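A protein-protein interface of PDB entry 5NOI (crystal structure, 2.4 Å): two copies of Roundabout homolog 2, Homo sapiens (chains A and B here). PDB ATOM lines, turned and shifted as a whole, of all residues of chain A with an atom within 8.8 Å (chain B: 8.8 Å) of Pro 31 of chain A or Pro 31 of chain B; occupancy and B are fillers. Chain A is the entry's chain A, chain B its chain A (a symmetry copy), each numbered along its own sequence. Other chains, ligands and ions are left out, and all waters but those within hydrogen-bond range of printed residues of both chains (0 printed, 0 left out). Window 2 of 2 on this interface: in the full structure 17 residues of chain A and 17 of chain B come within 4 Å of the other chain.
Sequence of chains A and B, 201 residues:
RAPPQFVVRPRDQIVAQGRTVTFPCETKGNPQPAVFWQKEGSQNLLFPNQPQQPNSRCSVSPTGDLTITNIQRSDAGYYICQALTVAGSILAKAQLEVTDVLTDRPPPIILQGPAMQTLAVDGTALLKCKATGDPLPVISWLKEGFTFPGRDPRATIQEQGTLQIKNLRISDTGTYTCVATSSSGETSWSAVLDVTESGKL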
ATOM      1  N   ARG A   1     -15.497 -22.584   4.366  1.00  0.00           N
ATOM      2  CA  ARG A   1     -14.454 -21.839   3.673  1.00  0.00           C
ATOM      3  C   ARG A   1     -14.002 -22.431   2.330  1.00  0.00           C
ATOM      4  O   ARG A   1     -13.261 -21.768   1.582  1.00  0.00           O
ATOM      5  CB  ARG A   1     -13.233 -21.712   4.575  1.00  0.00           C
ATOM      6  CG  ARG A   1     -12.500 -23.009   4.801  1.00  0.00           C
ATOM      7  CD  ARG A   1     -11.316 -22.795   5.731  1.00  0.00           C
ATOM      8  NE  ARG A   1     -11.738 -22.605   7.120  1.00  0.00           N
ATOM      9  CZ  ARG A   1     -12.018 -21.430   7.683  1.00  0.00           C
ATOM     10  NH1 ARG A   1     -11.924 -20.303   6.987  1.00  0.00           N
ATOM     11  NH2 ARG A   1     -12.392 -21.381   8.954  1.00  0.00           N
ATOM     12  N   ALA A   2     -14.420 -23.658   2.019  1.00  0.00           N
ATOM     13  CA  ALA A   2     -14.040 -24.325   0.768  1.00  0.00           C
ATOM     14  C   ALA A   2     -15.277 -24.863   0.068  1.00  0.00           C
ATOM     15  O   ALA A   2     -15.878 -25.847   0.570  1.00  0.00           O
ATOM     16  CB  ALA A   2     -13.037 -25.450   1.016  1.00  0.00           C
ATOM     17  N   PRO A   3     -15.653 -24.335  -1.092  1.00  0.00           N
ATOM     18  CA  PRO A   3     -16.902 -24.729  -1.753  1.00  0.00           C
ATOM     19  C   PRO A   3     -16.958 -26.229  -1.993  1.00  0.00           C
ATOM     20  O   PRO A   3     -15.922 -26.895  -2.153  1.00  0.00           O
ATOM     21  CB  PRO A   3     -16.863 -23.970  -3.089  1.00  0.00           C
ATOM     22  CG  PRO A   3     -15.847 -22.907  -2.919  1.00  0.00           C
ATOM     23  CD  PRO A   3     -14.844 -23.445  -1.949  1.00  0.00           C
ATOM     24  N   PRO A   4     -18.156 -26.798  -2.025  1.00  0.00           N
ATOM     25  CA  PRO A   4     -18.271 -28.221  -2.342  1.00  0.00           C
ATOM     26  C   PRO A   4     -17.849 -28.482  -3.780  1.00  0.00           C
ATOM     27  O   PRO A   4     -18.043 -27.656  -4.674  1.00  0.00           O
ATOM     28  CB  PRO A   4     -19.764 -28.515  -2.117  1.00  0.00           C
ATOM     29  CG  PRO A   4     -20.245 -27.391  -1.222  1.00  0.00           C
ATOM     30  CD  PRO A   4     -19.460 -26.204  -1.706  1.00  0.00           C
ATOM     31  N   GLN A   5     -17.254 -29.653  -3.973  1.00  0.00           N
ATOM     32  CA  GLN A   5     -16.784 -30.146  -5.254  1.00  0.00           C
ATOM     33  C   GLN A   5     -17.038 -31.643  -5.297  1.00  0.00           C
ATOM     34  O   GLN A   5     -17.020 -32.317  -4.262  1.00  0.00           O
ATOM     35  CB  GLN A   5     -15.267 -29.942  -5.473  1.00  0.00           C
ATOM     36  CG  GLN A   5     -14.709 -28.535  -5.505  1.00  0.00           C
ATOM     37  CD  GLN A   5     -13.172 -28.587  -5.628  1.00  0.00           C
ATOM     38  OE1 GLN A   5     -12.631 -29.267  -6.510  1.00  0.00           O
ATOM     39  NE2 GLN A   5     -12.473 -27.902  -4.722  1.00  0.00           N
ATOM     40  N   THR A  27     -18.063 -36.575  -2.496  1.00  0.00           N
ATOM     41  CA  THR A  27     -18.058 -35.136  -2.407  1.00  0.00           C
ATOM     42  C   THR A  27     -16.964 -34.693  -1.434  1.00  0.00           C
ATOM     43  O   THR A  27     -16.530 -35.459  -0.569  1.00  0.00           O
ATOM     44  CB  THR A  27     -19.456 -34.684  -1.996  1.00  0.00           C
ATOM     45  OG1 THR A  27     -19.469 -33.278  -1.770  1.00  0.00           O
ATOM     46  CG2 THR A  27     -19.898 -35.445  -0.728  1.00  0.00           C
ATOM     47  N   LYS A  28     -16.493 -33.456  -1.610  1.00  0.00           N
ATOM     48  CA  LYS A  28     -15.479 -32.899  -0.719  1.00  0.00           C
ATOM     49  C   LYS A  28     -15.727 -31.410  -0.537  1.00  0.00           C
ATOM     50  O   LYS A  28     -16.372 -30.755  -1.367  1.00  0.00           O
ATOM     51  CB  LYS A  28     -14.050 -33.131  -1.248  1.00  0.00           C
ATOM     52  CG  LYS A  28     -13.643 -32.240  -2.422  1.00  0.00           C
ATOM     53  CD  LYS A  28     -12.292 -32.725  -2.989  1.00  0.00           C
ATOM     54  CE  LYS A  28     -11.835 -31.935  -4.214  1.00  0.00           C
ATOM     55  NZ  LYS A  28     -10.508 -32.436  -4.673  1.00  0.00           N
ATOM     56  N   GLY A  29     -15.198 -30.880   0.553  1.00  0.00           N
ATOM     57  CA  GLY A  29     -15.290 -29.459   0.816  1.00  0.00           C
ATOM     58  C   GLY A  29     -15.257 -29.190   2.311  1.00  0.00           C
ATOM     59  O   GLY A  29     -15.154 -30.098   3.133  1.00  0.00           O
ATOM     60  N   ASN A  30     -15.343 -27.909   2.631  1.00  0.00           N
ATOM     61  CA  ASN A  30     -15.362 -27.608   4.050  1.00  0.00           C
ATOM     62  C   ASN A  30     -16.299 -26.428   4.255  1.00  0.00           C
ATOM     63  O   ASN A  30     -15.976 -25.302   3.863  1.00  0.00           O
ATOM     64  CB  ASN A  30     -13.945 -27.298   4.555  1.00  0.00           C
ATOM     65  CG  ASN A  30     -13.891 -27.048   6.014  1.00  0.00           C
ATOM     66  OD1 ASN A  30     -14.830 -26.571   6.586  1.00  0.00           O
ATOM     67  ND2 ASN A  30     -12.789 -27.375   6.626  1.00  0.00           N
ATOM     68  N   PRO A  31     -17.334 -26.800   5.027  1.00  0.00           N
ATOM     69  CA  PRO A  31     -17.525 -28.109   5.680  1.00  0.00           C
ATOM     70  C   PRO A  31     -17.827 -29.274   4.722  1.00  0.00           C
ATOM     71  O   PRO A  31     -18.091 -29.025   3.544  1.00  0.00           O
ATOM     72  CB  PRO A  31     -18.714 -27.860   6.604  1.00  0.00           C
ATOM     73  CG  PRO A  31     -19.434 -26.677   6.012  1.00  0.00           C
ATOM     74  CD  PRO A  31     -18.387 -25.826   5.391  1.00  0.00           C
ATOM     75  N   GLN A  32     -17.749 -30.506   5.231  1.00  0.00           N
ATOM     76  CA  GLN A  32     -17.959 -31.700   4.425  1.00  0.00           C
ATOM     77  C   GLN A  32     -19.394 -31.728   3.899  1.00  0.00           C
ATOM     78  O   GLN A  32     -20.336 -31.794   4.699  1.00  0.00           O
ATOM     79  CB  GLN A  32     -17.653 -32.969   5.237  1.00  0.00           C
ATOM     80  CG  GLN A  32     -17.996 -34.305   4.574  1.00  0.00           C
ATOM     81  CD  GLN A  32     -17.308 -34.604   3.236  1.00  0.00           C
ATOM     82  OE1 GLN A  32     -16.185 -34.350   3.048  1.00  0.00           O
ATOM     83  NE2 GLN A  32     -17.981 -35.126   2.315  1.00  0.00           N
ATOM     84  N   PRO A  33     -19.596 -31.683   2.581  1.00  0.00           N
ATOM     85  CA  PRO A  33     -20.968 -31.636   2.053  1.00  0.00           C
ATOM     86  C   PRO A  33     -21.720 -32.918   2.356  1.00  0.00           C
ATOM     87  O   PRO A  33     -21.188 -34.026   2.237  1.00  0.00           O
ATOM     88  CB  PRO A  33     -20.764 -31.441   0.549  1.00  0.00           C
ATOM     89  CG  PRO A  33     -19.352 -30.831   0.448  1.00  0.00           C
ATOM     90  CD  PRO A  33     -18.585 -31.504   1.522  1.00  0.00           C
ATOM     91  N   ALA A  34     -22.967 -32.748   2.792  1.00  0.00           N
ATOM     92  CA  ALA A  34     -23.883 -33.856   3.029  1.00  0.00           C
ATOM     93  C   ALA A  34     -24.802 -33.965   1.804  1.00  0.00           C
ATOM     94  O   ALA A  34     -25.622 -33.074   1.557  1.00  0.00           O
ATOM     95  CB  ALA A  34     -24.661 -33.623   4.326  1.00  0.00           C
ATOM     96  N   ALA A  83     -25.951 -31.005  -2.846  1.00  0.00           N
ATOM     97  CA  ALA A  83     -25.261 -30.737  -1.594  1.00  0.00           C
ATOM     98  C   ALA A  83     -25.234 -29.243  -1.392  1.00  0.00           C
ATOM     99  O   ALA A  83     -24.916 -28.507  -2.331  1.00  0.00           O
ATOM    100  CB  ALA A  83     -23.845 -31.292  -1.605  1.00  0.00           C
ATOM    101  N   LEU A  84     -25.550 -28.801  -0.174  1.00  0.00           N
ATOM    102  CA  LEU A  84     -25.575 -27.388   0.185  1.00  0.00           C
ATOM    103  C   LEU A  84     -24.807 -27.193   1.493  1.00  0.00           C
ATOM    104  O   LEU A  84     -25.049 -27.908   2.474  1.00  0.00           O
ATOM    105  CB  LEU A  84     -27.022 -26.896   0.282  1.00  0.00           C
ATOM    106  CG  LEU A  84     -27.351 -25.532   0.790  1.00  0.00           C
ATOM    107  CD1 LEU A  84     -26.582 -24.483   0.121  1.00  0.00           C
ATOM    108  CD2 LEU A  84     -28.814 -25.241   0.647  1.00  0.00           C
ATOM    109  N   THR A  85     -23.801 -26.312   1.492  1.00  0.00           N
ATOM    110  CA  THR A  85     -23.071 -25.847   2.671  1.00  0.00           C
ATOM    111  C   THR A  85     -23.158 -24.330   2.696  1.00  0.00           C
ATOM    112  O   THR A  85     -23.693 -23.698   1.773  1.00  0.00           O
ATOM    113  CB  THR A  85     -21.587 -26.269   2.687  1.00  0.00           C
ATOM    114  OG1 THR A  85     -20.833 -25.415   1.816  1.00  0.00           O
ATOM    115  CG2 THR A  85     -21.405 -27.713   2.289  1.00  0.00           C
ATOM    116  N   VAL A  86     -22.646 -23.726   3.776  1.00  0.00           N
ATOM    117  CA  VAL A  86     -22.498 -22.275   3.758  1.00  0.00           C
ATOM    118  C   VAL A  86     -21.474 -21.816   2.729  1.00  0.00           C
ATOM    119  O   VAL A  86     -21.458 -20.627   2.398  1.00  0.00           O
ATOM    120  CB  VAL A  86     -22.155 -21.696   5.147  1.00  0.00           C
ATOM    121  CG1 VAL A  86     -23.439 -21.547   5.967  1.00  0.00           C
ATOM    122  CG2 VAL A  86     -21.110 -22.547   5.880  1.00  0.00           C
ATOM    123  N   ALA A  87     -20.674 -22.736   2.162  1.00  0.00           N
ATOM    124  CA  ALA A  87     -19.654 -22.390   1.166  1.00  0.00           C
ATOM    125  C   ALA A  87     -20.132 -22.486  -0.282  1.00  0.00           C
ATOM    126  O   ALA A  87     -19.595 -21.768  -1.132  1.00  0.00           O
ATOM    127  CB  ALA A  87     -18.412 -23.279   1.324  1.00  0.00           C
ATOM    128  N   GLY A  88     -21.101 -23.344  -0.591  1.00  0.00           N
ATOM    129  CA  GLY A  88     -21.635 -23.392  -1.942  1.00  0.00           C
ATOM    130  C   GLY A  88     -22.547 -24.590  -2.162  1.00  0.00           C
ATOM    131  O   GLY A  88     -22.798 -25.388  -1.251  1.00  0.00           O
ATOM    132  N   ARG B   1     -20.245 -31.992  14.196  1.00  0.00           N
ATOM    133  CA  ARG B   1     -20.317 -32.545  15.543  1.00  0.00           C
ATOM    134  C   ARG B   1     -21.532 -32.104  16.373  1.00  0.00           C
ATOM    135  O   ARG B   1     -21.777 -32.669  17.454  1.00  0.00           O
ATOM    136  CB  ARG B   1     -19.054 -32.179  16.313  1.00  0.00           C
ATOM    137  CG  ARG B   1     -18.946 -30.715  16.652  1.00  0.00           C
ATOM    138  CD  ARG B   1     -17.647 -30.437  17.393  1.00  0.00           C
ATOM    139  NE  ARG B   1     -16.488 -30.480  16.501  1.00  0.00           N
ATOM    140  CZ  ARG B   1     -15.762 -31.567  16.237  1.00  0.00           C
ATOM    141  NH1 ARG B   1     -16.059 -32.734  16.797  1.00  0.00           N
ATOM    142  NH2 ARG B   1     -14.730 -31.485  15.408  1.00  0.00           N
ATOM    143  N   ALA B   2     -22.282 -31.109  15.899  1.00  0.00           N
ATOM    144  CA  ALA B   2     -23.457 -30.600  16.613  1.00  0.00           C
ATOM    145  C   ALA B   2     -24.653 -30.544  15.678  1.00  0.00           C
ATOM    146  O   ALA B   2     -24.666 -29.683  14.761  1.00  0.00           O
ATOM    147  CB  ALA B   2     -23.192 -29.223  17.220  1.00  0.00           C
ATOM    148  N   PRO B   3     -25.687 -31.352  15.888  1.00  0.00           N
ATOM    149  CA  PRO B   3     -26.812 -31.429  14.951  1.00  0.00           C
ATOM    150  C   PRO B   3     -27.447 -30.066  14.726  1.00  0.00           C
ATOM    151  O   PRO B   3     -27.416 -29.189  15.605  1.00  0.00           O
ATOM    152  CB  PRO B   3     -27.802 -32.377  15.647  1.00  0.00           C
ATOM    153  CG  PRO B   3     -27.020 -33.083  16.687  1.00  0.00           C
ATOM    154  CD  PRO B   3     -25.947 -32.133  17.114  1.00  0.00           C
ATOM    155  N   PRO B   4     -28.035 -29.851  13.557  1.00  0.00           N
ATOM    156  CA  PRO B   4     -28.738 -28.591  13.324  1.00  0.00           C
ATOM    157  C   PRO B   4     -29.960 -28.489  14.223  1.00  0.00           C
ATOM    158  O   PRO B   4     -30.614 -29.483  14.547  1.00  0.00           O
ATOM    159  CB  PRO B   4     -29.122 -28.669  11.835  1.00  0.00           C
ATOM    160  CG  PRO B   4     -28.179 -29.701  11.251  1.00  0.00           C
ATOM    161  CD  PRO B   4     -28.033 -30.704  12.362  1.00  0.00           C
ATOM    162  N   GLN B   5     -30.244 -27.256  14.626  1.00  0.00           N
ATOM    163  CA  GLN B   5     -31.370 -26.893  15.464  1.00  0.00           C
ATOM    164  C   GLN B   5     -31.894 -25.550  14.984  1.00  0.00           C
ATOM    165  O   GLN B   5     -31.133 -24.721  14.474  1.00  0.00           O
ATOM    166  CB  GLN B   5     -30.997 -26.722  16.956  1.00  0.00           C
ATOM    167  CG  GLN B   5     -30.462 -27.912  17.723  1.00  0.00           C
ATOM    168  CD  GLN B   5     -30.064 -27.477  19.148  1.00  0.00           C
ATOM    169  OE1 GLN B   5     -30.856 -26.846  19.862  1.00  0.00           O
ATOM    170  NE2 GLN B   5     -28.826 -27.777  19.546  1.00  0.00           N
ATOM    171  N   THR B  27     -31.028 -20.650  12.077  1.00  0.00           N
ATOM    172  CA  THR B  27     -30.563 -21.996  12.304  1.00  0.00           C
ATOM    173  C   THR B  27     -29.196 -21.950  12.987  1.00  0.00           C
ATOM    174  O   THR B  27     -28.471 -20.954  12.901  1.00  0.00           O
ATOM    175  CB  THR B  27     -30.549 -22.722  10.962  1.00  0.00           C
ATOM    176  OG1 THR B  27     -29.974 -24.017  11.113  1.00  0.00           O
ATOM    177  CG2 THR B  27     -29.758 -21.892   9.929  1.00  0.00           C
ATOM    178  N   LYS B  28     -28.865 -23.028  13.702  1.00  0.00           N
ATOM    179  CA  LYS B  28     -27.568 -23.127  14.366  1.00  0.00           C
ATOM    180  C   LYS B  28     -27.093 -24.571  14.337  1.00  0.00           C
ATOM    181  O   LYS B  28     -27.887 -25.511  14.199  1.00  0.00           O
ATOM    182  CB  LYS B  28     -27.621 -22.622  15.823  1.00  0.00           C
ATOM    183  CG  LYS B  28     -28.304 -23.567  16.809  1.00  0.00           C
ATOM    184  CD  LYS B  28     -28.484 -22.850  18.164  1.00  0.00           C
ATOM    185  CE  LYS B  28     -29.224 -23.696  19.200  1.00  0.00           C
ATOM    186  NZ  LYS B  28     -29.319 -22.951  20.487  1.00  0.00           N
ATOM    187  N   GLY B  29     -25.788 -24.737  14.480  1.00  0.00           N
ATOM    188  CA  GLY B  29     -25.205 -26.060  14.549  1.00  0.00           C
ATOM    189  C   GLY B  29     -23.773 -26.039  14.039  1.00  0.00           C
ATOM    190  O   GLY B  29     -23.238 -25.004  13.646  1.00  0.00           O
ATOM    191  N   ASN B  30     -23.173 -27.218  14.065  1.00  0.00           N
ATOM    192  CA  ASN B  30     -21.820 -27.254  13.543  1.00  0.00           C
ATOM    193  C   ASN B  30     -21.641 -28.584  12.830  1.00  0.00           C
ATOM    194  O   ASN B  30     -21.585 -29.635  13.476  1.00  0.00           O
ATOM    195  CB  ASN B  30     -20.800 -27.081  14.679  1.00  0.00           C
ATOM    196  CG  ASN B  30     -19.399 -27.042  14.199  1.00  0.00           C
ATOM    197  OD1 ASN B  30     -19.077 -27.641  13.213  1.00  0.00           O
ATOM    198  ND2 ASN B  30     -18.559 -26.329  14.893  1.00  0.00           N
ATOM    199  N   PRO B  31     -21.395 -28.369  11.527  1.00  0.00           N
ATOM    200  CA  PRO B  31     -21.220 -27.063  10.862  1.00  0.00           C
ATOM    201  C   PRO B  31     -22.496 -26.211  10.758  1.00  0.00           C
ATOM    202  O   PRO B  31     -23.583 -26.728  11.028  1.00  0.00           O
ATOM    203  CB  PRO B  31     -20.726 -27.450   9.472  1.00  0.00           C
ATOM    204  CG  PRO B  31     -21.189 -28.868   9.267  1.00  0.00           C
ATOM    205  CD  PRO B  31     -21.167 -29.507  10.607  1.00  0.00           C
ATOM    206  N   GLN B  32     -22.339 -24.932  10.409  1.00  0.00           N
ATOM    207  CA  GLN B  32     -23.455 -24.001  10.322  1.00  0.00           C
ATOM    208  C   GLN B  32     -24.425 -24.451   9.229  1.00  0.00           C
ATOM    209  O   GLN B  32     -24.041 -24.496   8.053  1.00  0.00           O
ATOM    210  CB  GLN B  32     -22.956 -22.573  10.052  1.00  0.00           C
ATOM    211  CG  GLN B  32     -24.025 -21.517   9.763  1.00  0.00           C
ATOM    212  CD  GLN B  32     -25.077 -21.290  10.857  1.00  0.00           C
ATOM    213  OE1 GLN B  32     -24.797 -21.266  11.989  1.00  0.00           O
ATOM    214  NE2 GLN B  32     -26.275 -21.139  10.518  1.00  0.00           N
ATOM    215  N   PRO B  33     -25.670 -24.783   9.573  1.00  0.00           N
ATOM    216  CA  PRO B  33     -26.601 -25.287   8.552  1.00  0.00           C
ATOM    217  C   PRO B  33     -26.924 -24.218   7.525  1.00  0.00           C
ATOM    218  O   PRO B  33     -27.145 -23.049   7.854  1.00  0.00           O
ATOM    219  CB  PRO B  33     -27.836 -25.686   9.362  1.00  0.00           C
ATOM    220  CG  PRO B  33     -27.284 -25.907  10.784  1.00  0.00           C
ATOM    221  CD  PRO B  33     -26.233 -24.873  10.934  1.00  0.00           C
ATOM    222  N   ALA B  34     -26.910 -24.633   6.260  1.00  0.00           N
ATOM    223  CA  ALA B  34     -27.303 -23.785   5.142  1.00  0.00           C
ATOM    224  C   ALA B  34     -28.749 -24.145   4.775  1.00  0.00           C
ATOM    225  O   ALA B  34     -29.014 -25.251   4.292  1.00  0.00           O
ATOM    226  CB  ALA B  34     -26.336 -23.980   3.972  1.00  0.00           C
ATOM    227  N   ALA B  83     -32.548 -28.086   6.097  1.00  0.00           N
ATOM    228  CA  ALA B  83     -31.111 -27.932   6.275  1.00  0.00           C
ATOM    229  C   ALA B  83     -30.523 -29.305   6.487  1.00  0.00           C
ATOM    230  O   ALA B  83     -31.067 -30.085   7.276  1.00  0.00           O
ATOM    231  CB  ALA B  83     -30.788 -27.033   7.457  1.00  0.00           C
ATOM    232  N   LEU B  84     -29.416 -29.589   5.803  1.00  0.00           N
ATOM    233  CA  LEU B  84     -28.724 -30.870   5.892  1.00  0.00           C
ATOM    234  C   LEU B  84     -27.231 -30.617   6.104  1.00  0.00           C
ATOM    235  O   LEU B  84     -26.619 -29.828   5.373  1.00  0.00           O
ATOM    236  CB  LEU B  84     -28.998 -31.704   4.637  1.00  0.00           C
ATOM    237  CG  LEU B  84     -28.289 -32.993   4.384  1.00  0.00           C
ATOM    238  CD1 LEU B  84     -28.351 -33.901   5.528  1.00  0.00           C
ATOM    239  CD2 LEU B  84     -28.838 -33.682   3.173  1.00  0.00           C
ATOM    240  N   THR B  85     -26.655 -31.184   7.170  1.00  0.00           N
ATOM    241  CA  THR B  85     -25.220 -31.219   7.450  1.00  0.00           C
ATOM    242  C   THR B  85     -24.824 -32.675   7.632  1.00  0.00           C
ATOM    243  O   THR B  85     -25.669 -33.581   7.624  1.00  0.00           O
ATOM    244  CB  THR B  85     -24.813 -30.422   8.706  1.00  0.00           C
ATOM    245  OG1 THR B  85     -25.114 -31.187   9.880  1.00  0.00           O
ATOM    246  CG2 THR B  85     -25.493 -29.077   8.767  1.00  0.00           C
ATOM    247  N   VAL B  86     -23.514 -32.918   7.776  1.00  0.00           N
ATOM    248  CA  VAL B  86     -23.095 -34.256   8.178  1.00  0.00           C
ATOM    249  C   VAL B  86     -23.552 -34.603   9.587  1.00  0.00           C
ATOM    250  O   VAL B  86     -23.528 -35.784   9.945  1.00  0.00           O
ATOM    251  CB  VAL B  86     -21.571 -34.464   8.045  1.00  0.00           C
ATOM    252  CG1 VAL B  86     -21.230 -34.800   6.591  1.00  0.00           C
ATOM    253  CG2 VAL B  86     -20.780 -33.249   8.546  1.00  0.00           C
ATOM    254  N   ALA B  87     -24.036 -33.619  10.367  1.00  0.00           N
ATOM    255  CA  ALA B  87     -24.494 -33.854  11.740  1.00  0.00           C
ATOM    256  C   ALA B  87     -25.989 -34.150  11.861  1.00  0.00           C
ATOM    257  O   ALA B  87     -26.382 -34.839  12.809  1.00  0.00           O
ATOM    258  CB  ALA B  87     -24.166 -32.653  12.639  1.00  0.00           C
ATOM    259  N   GLY B  88     -26.825 -33.650  10.955  1.00  0.00           N
ATOM    260  CA  GLY B  88     -28.239 -33.988  10.996  1.00  0.00           C
ATOM    261  C   GLY B  88     -29.066 -33.135  10.046  1.00  0.00           C
ATOM    262  O   GLY B  88     -28.541 -32.283   9.319  1.00  0.00           O
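O of Thr 27 of chain A sits at hydrogen-bond distance from NE2 of Gln 32 of chain A, at 3.2 Å.
The side-chain hydroxyl (OG1) of Thr 85 of chain A sits at hydrogen-bond distance from the backbone NH (N) of Ala 87 of chain A (2.7 Å).
The backbone NH of Gly 88 of chain A lies within hydrogen-bond range of the side-chain hydroxyl of Thr 85 of chain A (3.2 Å).
The backbone carbonyl oxygen of Thr 27 of chain B is in hydrogen-bond range of the side-chain amide nitrogen of Gln 32 of chain B (3.2 Å).
The backbone NH of Ala 87 of chain B lies within hydrogen-bond range of the side-chain hydroxyl of Thr 85 of chain B (2.7 Å).
The side-chain hydroxyl (OG1) of Thr 85 of chain B sits at hydrogen-bond distance from the backbone NH (N) of Gly 88 of chain B.
Among the printed residues, merely in contact across the chains: Thr 85 of chain A with Ala 34 of chain B, Ala 34 of chain A with Thr 85 of chain B, Pro 31 of chain A with Pro 31 of chain B, Ala 34 of chain A with Leu 84 of chain B, Leu 84 of chain A with Ala 34 of chain B, Val 86 of chain A with Gln 32 of chain B, Gln 32 of chain A with Val 86 of chain B, Ala 34 of chain A with Val 86 of chain B, Val 86 of chain A with Ala 34 of chain B and Leu 84 of chain A with Leu 84 of chain B.
Printed residues of chain B within 4 Å of Pro 31 of chain A: Pro 31 (3.5 Å).
Pro 31 of chain B touches just one residue of chain A: Pro 31.
No residue of chain B comes within 4 Å of Gly 29 of chain A.
Printed residues of chain A within 4 Å of Leu 84 of chain B: Ala 34 and Leu 84.
Printed residues of chain A within 4 Å of Gln 32 of chain B: Val 86.
The nearest residue of chain B that does not touch Pro 31 of chain A is Gln 32 of chain B (5.5 Å).
The nearest residue of chain A that does not touch Pro 31 of chain B is Gln 32 of chain A (5.5 Å).
Of the 19 printed residues of chain A, 6 touch a printed residue of chain B.
Hydrophobic or aromatic side chains of chain A that line the printed part of chain B: Pro 31, Ala 34, Leu 84 and Val 86.
Printed residues of chain B that touch a printed residue of chain A: Pro 31, Gln 32, Ala 34, Leu 84, Thr 85 and Val 86.
Among the printed residues, 10 pairs touch across the chains.
Among the printed residues, no Asp or Glu carboxylate lies within 4 Å of a Lys or Arg side-chain nitrogen of the other chain.
Gln 32 of chain A touches Val 86 of chain B, and with the chains exchanged Val 86 of chain A touches Gln 32 of chain B.
Ala 34 of chain A touches Leu 84 of chain B, and with the chains exchanged Leu 84 of chain A touches Ala 34 of chain B.
Ala 34 of chain A touches Thr 85 of chain B, and with the chains exchanged Thr 85 of chain A touches Ala 34 of chain B.
Ala 34 of chain A touches Val 86 of chain B, and with the chains exchanged Val 86 of chain A touches Ala 34 of chain B.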
